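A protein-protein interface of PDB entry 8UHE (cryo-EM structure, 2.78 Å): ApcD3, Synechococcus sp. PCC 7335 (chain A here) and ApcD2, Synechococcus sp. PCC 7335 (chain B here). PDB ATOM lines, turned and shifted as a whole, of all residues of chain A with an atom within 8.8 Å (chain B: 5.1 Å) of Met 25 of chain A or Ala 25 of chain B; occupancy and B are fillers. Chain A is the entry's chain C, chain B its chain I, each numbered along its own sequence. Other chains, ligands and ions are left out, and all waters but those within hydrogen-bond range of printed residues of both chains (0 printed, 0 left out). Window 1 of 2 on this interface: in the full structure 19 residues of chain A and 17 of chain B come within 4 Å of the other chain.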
ATOM      1  N   SER A   2      32.097  10.551  -3.902  1.00  0.00           N
ATOM      2  CA  SER A   2      30.927   9.686  -3.822  1.00  0.00           C
ATOM      3  C   SER A   2      31.045   8.725  -2.642  1.00  0.00           C
ATOM      4  O   SER A   2      31.975   8.824  -1.844  1.00  0.00           O
ATOM      5  CB  SER A   2      30.738   8.914  -5.130  1.00  0.00           C
ATOM      6  OG  SER A   2      31.839   8.065  -5.391  1.00  0.00           O
ATOM      7  N   ILE A   3      30.080   7.813  -2.520  1.00  0.00           N
ATOM      8  CA  ILE A   3      30.160   6.775  -1.495  1.00  0.00           C
ATOM      9  C   ILE A   3      31.259   5.778  -1.842  1.00  0.00           C
ATOM     10  O   ILE A   3      32.072   5.393  -0.988  1.00  0.00           O
ATOM     11  CB  ILE A   3      28.789   6.093  -1.333  1.00  0.00           C
ATOM     12  CG1 ILE A   3      27.776   7.070  -0.735  1.00  0.00           C
ATOM     13  CG2 ILE A   3      28.881   4.856  -0.463  1.00  0.00           C
ATOM     14  CD1 ILE A   3      28.332   7.910   0.401  1.00  0.00           C
ATOM     15  N   VAL A   4      31.313   5.370  -3.111  1.00  0.00           N
ATOM     16  CA  VAL A   4      32.337   4.433  -3.562  1.00  0.00           C
ATOM     17  C   VAL A   4      33.713   5.079  -3.500  1.00  0.00           C
ATOM     18  O   VAL A   4      34.703   4.422  -3.170  1.00  0.00           O
ATOM     19  CB  VAL A   4      32.012   3.932  -4.979  1.00  0.00           C
ATOM     20  CG1 VAL A   4      32.805   2.682  -5.281  1.00  0.00           C
ATOM     21  CG2 VAL A   4      30.520   3.678  -5.118  1.00  0.00           C
ATOM     22  N   GLN A   6      34.729   7.484  -1.324  1.00  0.00           N
ATOM     23  CA  GLN A   6      35.152   7.533   0.072  1.00  0.00           C
ATOM     24  C   GLN A   6      35.531   6.148   0.578  1.00  0.00           C
ATOM     25  O   GLN A   6      36.508   5.997   1.323  1.00  0.00           O
ATOM     26  CB  GLN A   6      34.042   8.141   0.931  1.00  0.00           C
ATOM     27  CG  GLN A   6      34.333   8.159   2.422  1.00  0.00           C
ATOM     28  CD  GLN A   6      35.454   9.110   2.789  1.00  0.00           C
ATOM     29  OE1 GLN A   6      35.283  10.327   2.768  1.00  0.00           O
ATOM     30  NE2 GLN A   6      36.610   8.554   3.134  1.00  0.00           N
ATOM     31  N   ILE A   7      34.790   5.122   0.154  1.00  0.00           N
ATOM     32  CA  ILE A   7      35.094   3.757   0.574  1.00  0.00           C
ATOM     33  C   ILE A   7      36.424   3.288  -0.009  1.00  0.00           C
ATOM     34  O   ILE A   7      37.237   2.678   0.693  1.00  0.00           O
ATOM     35  CB  ILE A   7      33.928   2.824   0.201  1.00  0.00           C
ATOM     36  CG1 ILE A   7      32.847   2.932   1.269  1.00  0.00           C
ATOM     37  CG2 ILE A   7      34.381   1.381   0.058  1.00  0.00           C
ATOM     38  CD1 ILE A   7      31.504   2.604   0.773  1.00  0.00           C
ATOM     39  N   ASN A  10      39.248   5.114   1.858  1.00  0.00           N
ATOM     40  CA  ASN A  10      39.433   4.564   3.197  1.00  0.00           C
ATOM     41  C   ASN A  10      40.004   3.151   3.166  1.00  0.00           C
ATOM     42  O   ASN A  10      40.746   2.768   4.078  1.00  0.00           O
ATOM     43  CB  ASN A  10      38.107   4.581   3.953  1.00  0.00           C
ATOM     44  CG  ASN A  10      37.997   5.755   4.895  1.00  0.00           C
ATOM     45  OD1 ASN A  10      36.991   6.463   4.912  1.00  0.00           O
ATOM     46  ND2 ASN A  10      39.040   5.972   5.690  1.00  0.00           N
ATOM     47  N   THR A  19      35.470  -3.948   3.097  1.00  0.00           N
ATOM     48  CA  THR A  19      34.817  -4.902   3.977  1.00  0.00           C
ATOM     49  C   THR A  19      33.393  -5.176   3.492  1.00  0.00           C
ATOM     50  O   THR A  19      32.872  -4.449   2.643  1.00  0.00           O
ATOM     51  CB  THR A  19      34.795  -4.360   5.407  1.00  0.00           C
ATOM     52  OG1 THR A  19      33.666  -3.496   5.576  1.00  0.00           O
ATOM     53  CG2 THR A  19      36.064  -3.597   5.726  1.00  0.00           C
ATOM     54  N   PRO A  20      32.748  -6.242   3.989  1.00  0.00           N
ATOM     55  CA  PRO A  20      31.344  -6.487   3.622  1.00  0.00           C
ATOM     56  C   PRO A  20      30.410  -5.358   4.011  1.00  0.00           C
ATOM     57  O   PRO A  20      29.401  -5.139   3.332  1.00  0.00           O
ATOM     58  CB  PRO A  20      30.988  -7.757   4.403  1.00  0.00           C
ATOM     59  CG  PRO A  20      32.195  -8.446   4.609  1.00  0.00           C
ATOM     60  CD  PRO A  20      33.331  -7.419   4.652  1.00  0.00           C
ATOM     61  N   GLY A  21      30.681  -4.631   5.085  1.00  0.00           N
ATOM     62  CA  GLY A  21      29.792  -3.535   5.397  1.00  0.00           C
ATOM     63  C   GLY A  21      29.925  -2.364   4.447  1.00  0.00           C
ATOM     64  O   GLY A  21      28.929  -1.712   4.137  1.00  0.00           O
ATOM     65  N   GLU A  22      31.141  -2.102   3.939  1.00  0.00           N
ATOM     66  CA  GLU A  22      31.298  -1.090   2.893  1.00  0.00           C
ATOM     67  C   GLU A  22      30.521  -1.473   1.642  1.00  0.00           C
ATOM     68  O   GLU A  22      29.887  -0.621   1.011  1.00  0.00           O
ATOM     69  CB  GLU A  22      32.771  -0.894   2.535  1.00  0.00           C
ATOM     70  CG  GLU A  22      33.731  -0.918   3.694  1.00  0.00           C
ATOM     71  CD  GLU A  22      33.347   0.045   4.784  1.00  0.00           C
ATOM     72  OE1 GLU A  22      33.101   1.231   4.480  1.00  0.00           O
ATOM     73  OE2 GLU A  22      33.278  -0.389   5.952  1.00  0.00           O
ATOM     74  N   LEU A  23      30.559  -2.752   1.270  1.00  0.00           N
ATOM     75  CA  LEU A  23      29.832  -3.195   0.090  1.00  0.00           C
ATOM     76  C   LEU A  23      28.325  -3.177   0.314  1.00  0.00           C
ATOM     77  O   LEU A  23      27.565  -2.933  -0.630  1.00  0.00           O
ATOM     78  CB  LEU A  23      30.314  -4.581  -0.322  1.00  0.00           C
ATOM     79  CG  LEU A  23      31.817  -4.561  -0.593  1.00  0.00           C
ATOM     80  CD1 LEU A  23      32.380  -5.891  -0.434  1.00  0.00           C
ATOM     81  CD2 LEU A  23      32.109  -4.030  -1.981  1.00  0.00           C
ATOM     82  N   GLU A  24      27.878  -3.404   1.552  1.00  0.00           N
ATOM     83  CA  GLU A  24      26.467  -3.199   1.870  1.00  0.00           C
ATOM     84  C   GLU A  24      26.078  -1.735   1.726  1.00  0.00           C
ATOM     85  O   GLU A  24      24.986  -1.420   1.234  1.00  0.00           O
ATOM     86  CB  GLU A  24      26.166  -3.702   3.284  1.00  0.00           C
ATOM     87  CG  GLU A  24      24.771  -4.307   3.456  1.00  0.00           C
ATOM     88  CD  GLU A  24      24.653  -5.710   2.883  1.00  0.00           C
ATOM     89  OE1 GLU A  24      23.606  -6.353   3.082  1.00  0.00           O
ATOM     90  OE2 GLU A  24      25.610  -6.189   2.249  1.00  0.00           O
ATOM     91  N   MET A  25      26.966  -0.830   2.145  1.00  0.00           N
ATOM     92  CA  MET A  25      26.739   0.600   1.958  1.00  0.00           C
ATOM     93  C   MET A  25      26.627   0.957   0.480  1.00  0.00           C
ATOM     94  O   MET A  25      25.729   1.708   0.074  1.00  0.00           O
ATOM     95  CB  MET A  25      27.872   1.382   2.620  1.00  0.00           C
ATOM     96  CG  MET A  25      27.496   2.732   3.189  1.00  0.00           C
ATOM     97  SD  MET A  25      28.939   3.820   3.106  1.00  0.00           S
ATOM     98  CE  MET A  25      28.350   5.346   3.806  1.00  0.00           C
ATOM     99  N   ILE A  26      27.527   0.404  -0.340  1.00  0.00           N
ATOM    100  CA  ILE A  26      27.511   0.662  -1.780  1.00  0.00           C
ATOM    101  C   ILE A  26      26.228   0.138  -2.409  1.00  0.00           C
ATOM    102  O   ILE A  26      25.604   0.816  -3.235  1.00  0.00           O
ATOM    103  CB  ILE A  26      28.758   0.053  -2.450  1.00  0.00           C
ATOM    104  CG1 ILE A  26      30.015   0.689  -1.865  1.00  0.00           C
ATOM    105  CG2 ILE A  26      28.702   0.235  -3.963  1.00  0.00           C
ATOM    106  CD1 ILE A  26      31.251   0.580  -2.683  1.00  0.00           C
ATOM    107  N   ARG A  27      25.806  -1.069  -2.022  1.00  0.00           N
ATOM    108  CA  ARG A  27      24.609  -1.653  -2.619  1.00  0.00           C
ATOM    109  C   ARG A  27      23.350  -0.905  -2.197  1.00  0.00           C
ATOM    110  O   ARG A  27      22.430  -0.730  -3.005  1.00  0.00           O
ATOM    111  CB  ARG A  27      24.518  -3.134  -2.259  1.00  0.00           C
ATOM    112  CG  ARG A  27      25.481  -3.988  -3.059  1.00  0.00           C
ATOM    113  CD  ARG A  27      25.257  -5.464  -2.826  1.00  0.00           C
ATOM    114  NE  ARG A  27      26.245  -6.018  -1.911  1.00  0.00           N
ATOM    115  CZ  ARG A  27      25.970  -6.438  -0.687  1.00  0.00           C
ATOM    116  NH1 ARG A  27      24.739  -6.396  -0.203  1.00  0.00           N
ATOM    117  NH2 ARG A  27      26.952  -6.909   0.076  1.00  0.00           N
ATOM    118  N   SER A  28      23.299  -0.432  -0.950  1.00  0.00           N
ATOM    119  CA  SER A  28      22.167   0.380  -0.517  1.00  0.00           C
ATOM    120  C   SER A  28      22.114   1.710  -1.265  1.00  0.00           C
ATOM    121  O   SER A  28      21.032   2.166  -1.671  1.00  0.00           O
ATOM    122  CB  SER A  28      22.245   0.610   0.990  1.00  0.00           C
ATOM    123  OG  SER A  28      22.410  -0.620   1.673  1.00  0.00           O
ATOM    124  N   PHE A  29      23.276   2.342  -1.469  1.00  0.00           N
ATOM    125  CA  PHE A  29      23.301   3.590  -2.225  1.00  0.00           C
ATOM    126  C   PHE A  29      22.896   3.369  -3.679  1.00  0.00           C
ATOM    127  O   PHE A  29      22.183   4.192  -4.262  1.00  0.00           O
ATOM    128  CB  PHE A  29      24.681   4.238  -2.156  1.00  0.00           C
ATOM    129  CG  PHE A  29      24.840   5.392  -3.098  1.00  0.00           C
ATOM    130  CD1 PHE A  29      24.029   6.510  -2.980  1.00  0.00           C
ATOM    131  CD2 PHE A  29      25.771   5.346  -4.121  1.00  0.00           C
ATOM    132  CE1 PHE A  29      24.153   7.563  -3.857  1.00  0.00           C
ATOM    133  CE2 PHE A  29      25.905   6.403  -4.998  1.00  0.00           C
ATOM    134  CZ  PHE A  29      25.097   7.513  -4.865  1.00  0.00           C
ATOM    135  N   CYS A  30      23.333   2.260  -4.279  1.00  0.00           N
ATOM    136  CA  CYS A  30      22.936   1.966  -5.653  1.00  0.00           C
ATOM    137  C   CYS A  30      21.446   1.653  -5.743  1.00  0.00           C
ATOM    138  O   CYS A  30      20.805   1.939  -6.763  1.00  0.00           O
ATOM    139  CB  CYS A  30      23.768   0.811  -6.207  1.00  0.00           C
ATOM    140  SG  CYS A  30      25.467   1.258  -6.636  1.00  0.00           S
ATOM    141  N   LYS A  31      20.880   1.062  -4.686  1.00  0.00           N
ATOM    142  CA  LYS A  31      19.436   0.855  -4.631  1.00  0.00           C
ATOM    143  C   LYS A  31      18.687   2.179  -4.604  1.00  0.00           C
ATOM    144  O   LYS A  31      17.654   2.332  -5.265  1.00  0.00           O
ATOM    145  CB  LYS A  31      19.070   0.019  -3.407  1.00  0.00           C
ATOM    146  CG  LYS A  31      18.458  -1.320  -3.748  1.00  0.00           C
ATOM    147  CD  LYS A  31      19.332  -2.069  -4.732  1.00  0.00           C
ATOM    148  CE  LYS A  31      18.517  -3.021  -5.583  1.00  0.00           C
ATOM    149  NZ  LYS A  31      19.400  -3.945  -6.343  1.00  0.00           N
ATOM    150  N   THR A  32      19.190   3.147  -3.842  1.00  0.00           N
ATOM    151  CA  THR A  32      18.563   4.465  -3.811  1.00  0.00           C
ATOM    152  C   THR A  32      18.994   5.360  -4.970  1.00  0.00           C
ATOM    153  O   THR A  32      18.542   6.510  -5.039  1.00  0.00           O
ATOM    154  CB  THR A  32      18.863   5.163  -2.483  1.00  0.00           C
ATOM    155  OG1 THR A  32      20.281   5.228  -2.286  1.00  0.00           O
ATOM    156  CG2 THR A  32      18.228   4.402  -1.334  1.00  0.00           C
ATOM    157  N   GLY A  96      26.140  10.862  -3.492  1.00  0.00           N
ATOM    158  CA  GLY A  96      25.802  10.203  -2.253  1.00  0.00           C
ATOM    159  C   GLY A  96      26.448  10.787  -1.021  1.00  0.00           C
ATOM    160  O   GLY A  96      26.181  10.298   0.080  1.00  0.00           O
ATOM    161  N   ASN A  97      27.296  11.800  -1.166  1.00  0.00           N
ATOM    162  CA  ASN A  97      27.846  12.507  -0.022  1.00  0.00           C
ATOM    163  C   ASN A  97      28.131  13.943  -0.440  1.00  0.00           C
ATOM    164  O   ASN A  97      27.883  14.341  -1.583  1.00  0.00           O
ATOM    165  CB  ASN A  97      29.098  11.812   0.527  1.00  0.00           C
ATOM    166  CG  ASN A  97      30.127  11.513  -0.545  1.00  0.00           C
ATOM    167  OD1 ASN A  97      29.997  11.939  -1.690  1.00  0.00           O
ATOM    168  ND2 ASN A  97      31.165  10.776  -0.171  1.00  0.00           N
ATOM    169  N   VAL B   3      28.995   0.657   9.726  1.00  0.00           N
ATOM    170  CA  VAL B   3      29.156   1.806   8.836  1.00  0.00           C
ATOM    171  C   VAL B   3      29.042   3.107   9.609  1.00  0.00           C
ATOM    172  O   VAL B   3      29.596   4.142   9.210  1.00  0.00           O
ATOM    173  CB  VAL B   3      28.166   1.705   7.650  1.00  0.00           C
ATOM    174  CG1 VAL B   3      26.845   2.203   7.898  1.00  0.00           C
ATOM    175  CG2 VAL B   3      28.703   2.447   6.486  1.00  0.00           C
ATOM    176  N   VAL B   7      31.676   6.229   9.550  1.00  0.00           N
ATOM    177  CA  VAL B   7      31.214   7.478   8.960  1.00  0.00           C
ATOM    178  C   VAL B   7      31.326   8.614   9.977  1.00  0.00           C
ATOM    179  O   VAL B   7      31.640   9.760   9.620  1.00  0.00           O
ATOM    180  CB  VAL B   7      29.797   7.294   8.377  1.00  0.00           C
ATOM    181  CG1 VAL B   7      28.679   7.413   9.417  1.00  0.00           C
ATOM    182  CG2 VAL B   7      29.601   8.209   7.213  1.00  0.00           C
ATOM    183  N   LYS B  20      24.185  14.891   4.791  1.00  0.00           N
ATOM    184  CA  LYS B  20      22.903  14.260   4.507  1.00  0.00           C
ATOM    185  C   LYS B  20      23.076  12.908   3.831  1.00  0.00           C
ATOM    186  O   LYS B  20      22.310  11.989   4.093  1.00  0.00           O
ATOM    187  CB  LYS B  20      22.042  15.207   3.662  1.00  0.00           C
ATOM    188  CG  LYS B  20      20.841  14.598   2.932  1.00  0.00           C
ATOM    189  CD  LYS B  20      19.740  14.039   3.853  1.00  0.00           C
ATOM    190  CE  LYS B  20      19.441  14.875   5.089  1.00  0.00           C
ATOM    191  NZ  LYS B  20      18.826  14.069   6.177  1.00  0.00           N
ATOM    192  N   GLY B  21      24.096  12.751   2.991  1.00  0.00           N
ATOM    193  CA  GLY B  21      24.328  11.452   2.376  1.00  0.00           C
ATOM    194  C   GLY B  21      24.754  10.392   3.375  1.00  0.00           C
ATOM    195  O   GLY B  21      24.284   9.250   3.330  1.00  0.00           O
ATOM    196  N   GLU B  22      25.636  10.766   4.303  1.00  0.00           N
ATOM    197  CA  GLU B  22      25.984   9.874   5.401  1.00  0.00           C
ATOM    198  C   GLU B  22      24.770   9.570   6.265  1.00  0.00           C
ATOM    199  O   GLU B  22      24.618   8.447   6.759  1.00  0.00           O
ATOM    200  CB  GLU B  22      27.088  10.501   6.239  1.00  0.00           C
ATOM    201  CG  GLU B  22      28.278  10.981   5.432  1.00  0.00           C
ATOM    202  CD  GLU B  22      29.144  11.933   6.219  1.00  0.00           C
ATOM    203  OE1 GLU B  22      28.904  13.151   6.139  1.00  0.00           O
ATOM    204  OE2 GLU B  22      30.059  11.471   6.935  1.00  0.00           O
ATOM    205  N   LEU B  23      23.890  10.560   6.441  1.00  0.00           N
ATOM    206  CA  LEU B  23      22.675  10.362   7.224  1.00  0.00           C
ATOM    207  C   LEU B  23      21.731   9.372   6.552  1.00  0.00           C
ATOM    208  O   LEU B  23      21.108   8.547   7.227  1.00  0.00           O
ATOM    209  CB  LEU B  23      21.983  11.702   7.455  1.00  0.00           C
ATOM    210  CG  LEU B  23      22.721  12.621   8.429  1.00  0.00           C
ATOM    211  CD1 LEU B  23      22.017  13.955   8.527  1.00  0.00           C
ATOM    212  CD2 LEU B  23      22.854  11.975   9.798  1.00  0.00           C
ATOM    213  N   ASP B  24      21.616   9.430   5.224  1.00  0.00           N
ATOM    214  CA  ASP B  24      20.828   8.429   4.508  1.00  0.00           C
ATOM    215  C   ASP B  24      21.477   7.056   4.578  1.00  0.00           C
ATOM    216  O   ASP B  24      20.778   6.038   4.639  1.00  0.00           O
ATOM    217  CB  ASP B  24      20.625   8.849   3.054  1.00  0.00           C
ATOM    218  CG  ASP B  24      20.173  10.275   2.926  1.00  0.00           C
ATOM    219  OD1 ASP B  24      19.918  10.891   3.979  1.00  0.00           O
ATOM    220  OD2 ASP B  24      20.080  10.782   1.788  1.00  0.00           O
ATOM    221  N   ALA B  25      22.808   7.009   4.561  1.00  0.00           N
ATOM    222  CA  ALA B  25      23.506   5.735   4.687  1.00  0.00           C
ATOM    223  C   ALA B  25      23.220   5.069   6.030  1.00  0.00           C
ATOM    224  O   ALA B  25      22.920   3.869   6.097  1.00  0.00           O
ATOM    225  CB  ALA B  25      24.993   5.961   4.508  1.00  0.00           C
ATOM    226  N   ILE B  26      23.267   5.845   7.113  1.00  0.00           N
ATOM    227  CA  ILE B  26      22.966   5.252   8.415  1.00  0.00           C
ATOM    228  C   ILE B  26      21.467   5.019   8.577  1.00  0.00           C
ATOM    229  O   ILE B  26      21.057   4.136   9.337  1.00  0.00           O
ATOM    230  CB  ILE B  26      23.524   6.104   9.573  1.00  0.00           C
ATOM    231  CG1 ILE B  26      23.246   7.554   9.388  1.00  0.00           C
ATOM    232  CG2 ILE B  26      24.942   6.367   9.389  1.00  0.00           C
ATOM    233  CD1 ILE B  26      24.015   8.479  10.356  1.00  0.00           C
ATOM    234  N   ASN B  27      20.632   5.797   7.881  1.00  0.00           N
ATOM    235  CA  ASN B  27      19.202   5.508   7.856  1.00  0.00           C
ATOM    236  C   ASN B  27      18.931   4.150   7.227  1.00  0.00           C
ATOM    237  O   ASN B  27      18.126   3.367   7.745  1.00  0.00           O
ATOM    238  CB  ASN B  27      18.457   6.600   7.089  1.00  0.00           C
ATOM    239  CG  ASN B  27      17.604   7.464   7.988  1.00  0.00           C
ATOM    240  OD1 ASN B  27      17.077   6.997   8.998  1.00  0.00           O
ATOM    241  ND2 ASN B  27      17.446   8.730   7.618  1.00  0.00           N
ATOM    242  N   ARG B  28      19.606   3.849   6.118  1.00  0.00           N
ATOM    243  CA  ARG B  28      19.466   2.537   5.495  1.00  0.00           C
ATOM    244  C   ARG B  28      20.040   1.437   6.382  1.00  0.00           C
ATOM    245  O   ARG B  28      19.512   0.318   6.399  1.00  0.00           O
ATOM    246  CB  ARG B  28      20.126   2.546   4.116  1.00  0.00           C
ATOM    247  CG  ARG B  28      19.390   3.441   3.125  1.00  0.00           C
ATOM    248  CD  ARG B  28      20.056   3.521   1.759  1.00  0.00           C
ATOM    249  NE  ARG B  28      21.463   3.897   1.811  1.00  0.00           N
ATOM    250  CZ  ARG B  28      21.995   4.888   1.108  1.00  0.00           C
ATOM    251  NH1 ARG B  28      21.250   5.675   0.348  1.00  0.00           N
ATOM    252  NH2 ARG B  28      23.307   5.097   1.170  1.00  0.00           N
ATOM    253  N   PHE B  29      21.093   1.750   7.143  1.00  0.00           N
ATOM    254  CA  PHE B  29      21.613   0.811   8.137  1.00  0.00           C
ATOM    255  C   PHE B  29      20.568   0.489   9.211  1.00  0.00           C
ATOM    256  O   PHE B  29      20.331  -0.686   9.541  1.00  0.00           O
ATOM    257  CB  PHE B  29      22.876   1.403   8.759  1.00  0.00           C
ATOM    258  CG  PHE B  29      23.518   0.530   9.784  1.00  0.00           C
ATOM    259  CD1 PHE B  29      24.281  -0.558   9.404  1.00  0.00           C
ATOM    260  CD2 PHE B  29      23.361   0.798  11.133  1.00  0.00           C
ATOM    261  CE1 PHE B  29      24.874  -1.359  10.352  1.00  0.00           C
ATOM    262  CE2 PHE B  29      23.952   0.004  12.083  1.00  0.00           C
ATOM    263  CZ  PHE B  29      24.706  -1.075  11.696  1.00  0.00           C
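The guanidinium group (NH1) of Arg 28 of chain B sits at hydrogen-bond distance from the side-chain hydroxyl (OG1) of Thr 32 of chain A (2.8 Å).
O of Ser 28 of chain A lies within hydrogen-bond range of OG1 of Thr 32 of chain A (3.2 Å).
The backbone carbonyl oxygen of Phe 29 of chain A is in hydrogen-bond range of the side-chain hydroxyl of Thr 32 of chain A (2.9 Å).
The side-chain hydroxyl (OG) of Ser 28 of chain A is in hydrogen-bond range of the backbone carbonyl oxygen (O) of Glu 24 of chain A (2.7 Å).
Among the printed residues, merely in contact across the chains: Gly 96 of chain A with Gly 21 of chain B (3.2 Å), Ser 28 of chain A with Arg 28 of chain B (3.5 Å), Met 25 of chain A with Ala 25 of chain B (3.5 Å), Met 25 of chain A with Val 3 of chain B (3.5 Å) and Phe 29 of chain A with Arg 28 of chain B (3.7 Å).
Of chain B, only Val 3 (3.5 Å) and Ala 25 (3.5 Å) come within 4 Å of Met 25 of chain A.
Of chain A, only Met 25 comes within 4 Å of Ala 25 of chain B.
Printed residues of chain B within 4 Å of Gly 96 of chain A: Gly 21.
Printed residues of chain A within 4 Å of Arg 28 of chain B: Ser 28, Phe 29 and Thr 32.
Of the printed residues of chain B, Ser 28 of chain A touches Arg 28 (3.5 Å).
Printed residues of chain A within 4 Å of Gly 21 of chain B: Gly 96 (3.2 Å).
Of the printed residues of chain B, Thr 32 of chain A touches Arg 28 (2.8 Å).
Printed residues of chain B that touch a printed residue of chain A: Val 3, Gly 21, Ala 25 and Arg 28.
Of the 22 printed residues of chain A, 5 touch a printed residue of chain B.
Hydrophobic or aromatic side chains of chain A that line the printed part of chain B: Met 25 and Phe 29.
Among the printed residues, no Asp or Glu carboxylate lies within 4 Å of a Lys or Arg side-chain nitrogen of the other chain.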
